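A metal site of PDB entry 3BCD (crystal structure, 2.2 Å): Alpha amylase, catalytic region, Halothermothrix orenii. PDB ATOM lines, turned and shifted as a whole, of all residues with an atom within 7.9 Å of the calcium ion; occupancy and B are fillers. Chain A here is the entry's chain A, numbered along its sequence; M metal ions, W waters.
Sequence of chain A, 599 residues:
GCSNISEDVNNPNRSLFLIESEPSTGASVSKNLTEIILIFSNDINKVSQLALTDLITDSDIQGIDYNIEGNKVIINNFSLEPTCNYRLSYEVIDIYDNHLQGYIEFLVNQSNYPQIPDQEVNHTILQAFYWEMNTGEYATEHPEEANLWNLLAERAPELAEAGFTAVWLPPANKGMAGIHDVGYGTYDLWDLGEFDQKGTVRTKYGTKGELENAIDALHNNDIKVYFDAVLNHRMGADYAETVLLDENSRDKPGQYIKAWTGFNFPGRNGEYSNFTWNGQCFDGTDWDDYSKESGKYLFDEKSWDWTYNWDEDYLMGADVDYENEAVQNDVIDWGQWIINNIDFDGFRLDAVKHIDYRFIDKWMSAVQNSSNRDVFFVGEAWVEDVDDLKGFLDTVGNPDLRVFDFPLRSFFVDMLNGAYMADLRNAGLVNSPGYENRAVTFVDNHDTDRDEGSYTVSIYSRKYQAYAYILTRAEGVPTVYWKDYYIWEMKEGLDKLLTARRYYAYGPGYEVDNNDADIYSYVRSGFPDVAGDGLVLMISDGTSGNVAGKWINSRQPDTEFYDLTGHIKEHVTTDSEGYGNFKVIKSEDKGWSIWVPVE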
ATOM      1  N   PHE A 411      21.601 -31.834  -1.684  1.00  0.00           N
ATOM      2  CA  PHE A 411      21.622 -30.907  -2.868  1.00  0.00           C
ATOM      3  C   PHE A 411      23.050 -30.378  -3.023  1.00  0.00           C
ATOM      4  O   PHE A 411      23.525 -30.240  -4.161  1.00  0.00           O
ATOM      5  CB  PHE A 411      20.707 -29.710  -2.759  1.00  0.00           C
ATOM      6  CG  PHE A 411      20.424 -29.037  -4.125  1.00  0.00           C
ATOM      7  CD1 PHE A 411      19.308 -29.407  -4.888  1.00  0.00           C
ATOM      8  CD2 PHE A 411      21.235 -28.091  -4.633  1.00  0.00           C
ATOM      9  CE1 PHE A 411      19.050 -28.806  -6.160  1.00  0.00           C
ATOM     10  CE2 PHE A 411      20.966 -27.477  -5.930  1.00  0.00           C
ATOM     11  CZ  PHE A 411      19.897 -27.823  -6.635  1.00  0.00           C
ATOM     12  N   MET A 415      25.455 -30.538  -6.281  1.00  0.00           N
ATOM     13  CA  MET A 415      26.248 -29.442  -6.863  1.00  0.00           C
ATOM     14  C   MET A 415      27.716 -29.794  -7.178  1.00  0.00           C
ATOM     15  O   MET A 415      28.322 -29.103  -7.900  1.00  0.00           O
ATOM     16  CB  MET A 415      26.246 -28.222  -5.964  1.00  0.00           C
ATOM     17  CG  MET A 415      24.926 -27.472  -5.948  1.00  0.00           C
ATOM     18  SD  MET A 415      24.694 -26.195  -4.698  1.00  0.00           S
ATOM     19  CE  MET A 415      26.088 -25.152  -5.027  1.00  0.00           C
ATOM     20  N   ASN A 417      29.152 -31.664  -9.114  1.00  0.00           N
ATOM     21  CA  ASN A 417      29.404 -31.810 -10.545  1.00  0.00           C
ATOM     22  C   ASN A 417      28.339 -31.089 -11.368  1.00  0.00           C
ATOM     23  O   ASN A 417      28.201 -31.346 -12.535  1.00  0.00           O
ATOM     24  CB  ASN A 417      29.517 -33.285 -10.943  1.00  0.00           C
ATOM     25  CG  ASN A 417      28.217 -34.010 -10.792  1.00  0.00           C
ATOM     26  OD1 ASN A 417      27.235 -33.432 -10.386  1.00  0.00           O
ATOM     27  ND2 ASN A 417      28.204 -35.269 -11.118  1.00  0.00           N
ATOM     28  N   GLY A 418      27.584 -30.198 -10.751  1.00  0.00           N
ATOM     29  CA  GLY A 418      26.579 -29.493 -11.489  1.00  0.00           C
ATOM     30  C   GLY A 418      25.214 -29.996 -11.100  1.00  0.00           C
ATOM     31  O   GLY A 418      24.947 -31.238 -11.174  1.00  0.00           O
ATOM     32  N   ALA A 419      24.397 -29.027 -10.630  1.00  0.00           N
ATOM     33  CA  ALA A 419      22.995 -29.198 -10.257  1.00  0.00           C
ATOM     34  C   ALA A 419      22.087 -28.266 -11.051  1.00  0.00           C
ATOM     35  O   ALA A 419      22.536 -27.341 -11.735  1.00  0.00           O
ATOM     36  CB  ALA A 419      22.808 -28.939  -8.751  1.00  0.00           C
ATOM     37  N   TYR A 420      20.799 -28.461 -10.924  1.00  0.00           N
ATOM     38  CA  TYR A 420      19.847 -27.548 -11.475  1.00  0.00           C
ATOM     39  C   TYR A 420      19.491 -26.499 -10.457  1.00  0.00           C
ATOM     40  O   TYR A 420      18.659 -26.728  -9.542  1.00  0.00           O
ATOM     41  CB  TYR A 420      18.600 -28.308 -11.927  1.00  0.00           C
ATOM     42  CG  TYR A 420      17.848 -27.510 -12.913  1.00  0.00           C
ATOM     43  CD1 TYR A 420      18.197 -27.536 -14.213  1.00  0.00           C
ATOM     44  CD2 TYR A 420      16.827 -26.663 -12.513  1.00  0.00           C
ATOM     45  CE1 TYR A 420      17.531 -26.813 -15.097  1.00  0.00           C
ATOM     46  CE2 TYR A 420      16.143 -25.915 -13.397  1.00  0.00           C
ATOM     47  CZ  TYR A 420      16.495 -25.983 -14.699  1.00  0.00           C
ATOM     48  OH  TYR A 420      15.808 -25.229 -15.607  1.00  0.00           O
ATOM     49  N   MET A 421      20.105 -25.324 -10.593  1.00  0.00           N
ATOM     50  CA  MET A 421      20.205 -24.426  -9.401  1.00  0.00           C
ATOM     51  C   MET A 421      18.865 -23.805  -8.955  1.00  0.00           C
ATOM     52  O   MET A 421      18.657 -23.610  -7.768  1.00  0.00           O
ATOM     53  CB  MET A 421      21.315 -23.378  -9.570  1.00  0.00           C
ATOM     54  CG  MET A 421      22.780 -23.913  -9.550  1.00  0.00           C
ATOM     55  SD  MET A 421      23.280 -24.537  -7.967  1.00  0.00           S
ATOM     56  CE  MET A 421      23.462 -22.991  -7.089  1.00  0.00           C
ATOM     57  N   ALA A 422      17.951 -23.598  -9.887  1.00  0.00           N
ATOM     58  CA  ALA A 422      16.579 -23.238  -9.614  1.00  0.00           C
ATOM     59  C   ALA A 422      15.873 -24.087  -8.562  1.00  0.00           C
ATOM     60  O   ALA A 422      15.016 -23.592  -7.847  1.00  0.00           O
ATOM     61  CB  ALA A 422      15.800 -23.294 -10.892  1.00  0.00           C
ATOM     62  N   ARG A 462      32.523 -25.787  -4.266  1.00  0.00           N
ATOM     63  CA  ARG A 462      31.330 -24.946  -4.066  1.00  0.00           C
ATOM     64  C   ARG A 462      30.811 -24.854  -2.641  1.00  0.00           C
ATOM     65  O   ARG A 462      29.651 -24.543  -2.381  1.00  0.00           O
ATOM     66  CB  ARG A 462      30.237 -25.346  -5.042  1.00  0.00           C
ATOM     67  CG  ARG A 462      30.734 -25.207  -6.512  1.00  0.00           C
ATOM     68  CD  ARG A 462      29.603 -25.291  -7.499  1.00  0.00           C
ATOM     69  NE  ARG A 462      30.089 -25.138  -8.863  1.00  0.00           N
ATOM     70  CZ  ARG A 462      30.605 -26.085  -9.627  1.00  0.00           C
ATOM     71  NH1 ARG A 462      30.745 -27.333  -9.178  1.00  0.00           N
ATOM     72  NH2 ARG A 462      31.027 -25.788 -10.877  1.00  0.00           N
ATOM     73  N   ASP A 516      17.717 -20.428 -12.964  1.00  0.00           N
ATOM     74  CA  ASP A 516      17.933 -21.358 -14.035  1.00  0.00           C
ATOM     75  C   ASP A 516      18.845 -22.528 -13.673  1.00  0.00           C
ATOM     76  O   ASP A 516      18.995 -22.935 -12.434  1.00  0.00           O
ATOM     77  CB  ASP A 516      18.386 -20.591 -15.322  1.00  0.00           C
ATOM     78  CG  ASP A 516      19.781 -19.927 -15.185  1.00  0.00           C
ATOM     79  OD1 ASP A 516      20.703 -20.523 -14.558  1.00  0.00           O
ATOM     80  OD2 ASP A 516      19.939 -18.815 -15.704  1.00  0.00           O
ATOM     81  N   ALA A 517      19.420 -23.147 -14.713  1.00  0.00           N
ATOM     82  CA  ALA A 517      20.237 -24.371 -14.480  1.00  0.00           C
ATOM     83  C   ALA A 517      21.409 -24.008 -13.643  1.00  0.00           C
ATOM     84  O   ALA A 517      21.856 -24.793 -12.778  1.00  0.00           O
ATOM     85  CB  ALA A 517      20.738 -25.008 -15.852  1.00  0.00           C
ATOM     86  N   ASP A 518      21.916 -22.799 -13.882  1.00  0.00           N
ATOM     87  CA  ASP A 518      23.139 -22.356 -13.202  1.00  0.00           C
ATOM     88  C   ASP A 518      23.141 -21.252 -12.165  1.00  0.00           C
ATOM     89  O   ASP A 518      24.110 -21.201 -11.407  1.00  0.00           O
ATOM     90  CB  ASP A 518      24.246 -22.129 -14.234  1.00  0.00           C
ATOM     91  CG  ASP A 518      24.336 -23.254 -15.230  1.00  0.00           C
ATOM     92  OD1 ASP A 518      24.097 -24.440 -14.864  1.00  0.00           O
ATOM     93  OD2 ASP A 518      24.590 -22.984 -16.423  1.00  0.00           O
ATOM     94  N   ILE A 519      22.089 -20.440 -12.056  1.00  0.00           N
ATOM     95  CA  ILE A 519      21.963 -19.352 -11.092  1.00  0.00           C
ATOM     96  C   ILE A 519      20.682 -19.436 -10.232  1.00  0.00           C
ATOM     97  O   ILE A 519      19.611 -19.626 -10.762  1.00  0.00           O
ATOM     98  CB  ILE A 519      21.960 -17.970 -11.776  1.00  0.00           C
ATOM     99  CG1 ILE A 519      23.295 -17.710 -12.520  1.00  0.00           C
ATOM    100  CG2 ILE A 519      21.785 -16.830 -10.760  1.00  0.00           C
ATOM    101  CD1 ILE A 519      23.329 -16.510 -13.454  1.00  0.00           C
ATOM    102  N   SER A 540      25.904 -19.444  -7.907  1.00  0.00           N
ATOM    103  CA  SER A 540      25.916 -20.058  -9.245  1.00  0.00           C
ATOM    104  C   SER A 540      26.806 -21.338  -9.255  1.00  0.00           C
ATOM    105  O   SER A 540      27.778 -21.424  -8.486  1.00  0.00           O
ATOM    106  CB  SER A 540      26.382 -19.051 -10.294  1.00  0.00           C
ATOM    107  OG  SER A 540      26.583 -19.701 -11.545  1.00  0.00           O
ATOM    108  N   ASP A 541      26.464 -22.334 -10.087  1.00  0.00           N
ATOM    109  CA  ASP A 541      27.389 -23.486 -10.365  1.00  0.00           C
ATOM    110  C   ASP A 541      28.088 -23.374 -11.714  1.00  0.00           C
ATOM    111  O   ASP A 541      28.727 -24.311 -12.160  1.00  0.00           O
ATOM    112  CB  ASP A 541      26.733 -24.870 -10.174  1.00  0.00           C
ATOM    113  CG  ASP A 541      25.655 -25.206 -11.214  1.00  0.00           C
ATOM    114  OD1 ASP A 541      25.176 -26.349 -11.209  1.00  0.00           O
ATOM    115  OD2 ASP A 541      25.266 -24.377 -12.056  1.00  0.00           O
ATOM    116  N   GLY A 542      28.016 -22.194 -12.307  1.00  0.00           N
ATOM    117  CA  GLY A 542      28.664 -21.933 -13.581  1.00  0.00           C
ATOM    118  C   GLY A 542      30.169 -21.981 -13.456  1.00  0.00           C
ATOM    119  O   GLY A 542      30.702 -21.797 -12.380  1.00  0.00           O
HETATM  120 CA    CA M   1      23.831 -25.944 -13.082  1.00  0.00          CA
HETATM  121  O   HOH W   1      25.639 -26.852 -13.742  1.00  0.00           O
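Along chain A the residues within 4 Å of the calcium ion span positions 419 to 541.
The nearest printed residue that does not touch the calcium ion is Met 421 (4.2 Å).
The side-chain hydroxyl of Ser 540 lies within hydrogen-bond range of the backbone carbonyl oxygen of Asp 518 (2.9 Å).
N of Asp 518 sits at hydrogen-bond distance from OD1 of Asp 516 (2.7 Å).
N of Met 421 sits close to O of Ala 517, 2.8 Å away.
The backbone carbonyl oxygen (O) of Asp 541 lies within hydrogen-bond range of the guanidinium group (NH2) of Arg 462, at 3.0 Å.
The calcium ion is bound by water W1 (2.1 Å), O of Ala 517 (2.3 Å), O of Ala 419 (2.3 Å), OD1 of Asp 541 (2.3 Å), OD1 of Asp 518 (2.3 Å) and OD2 of Asp 541 (2.4 Å).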
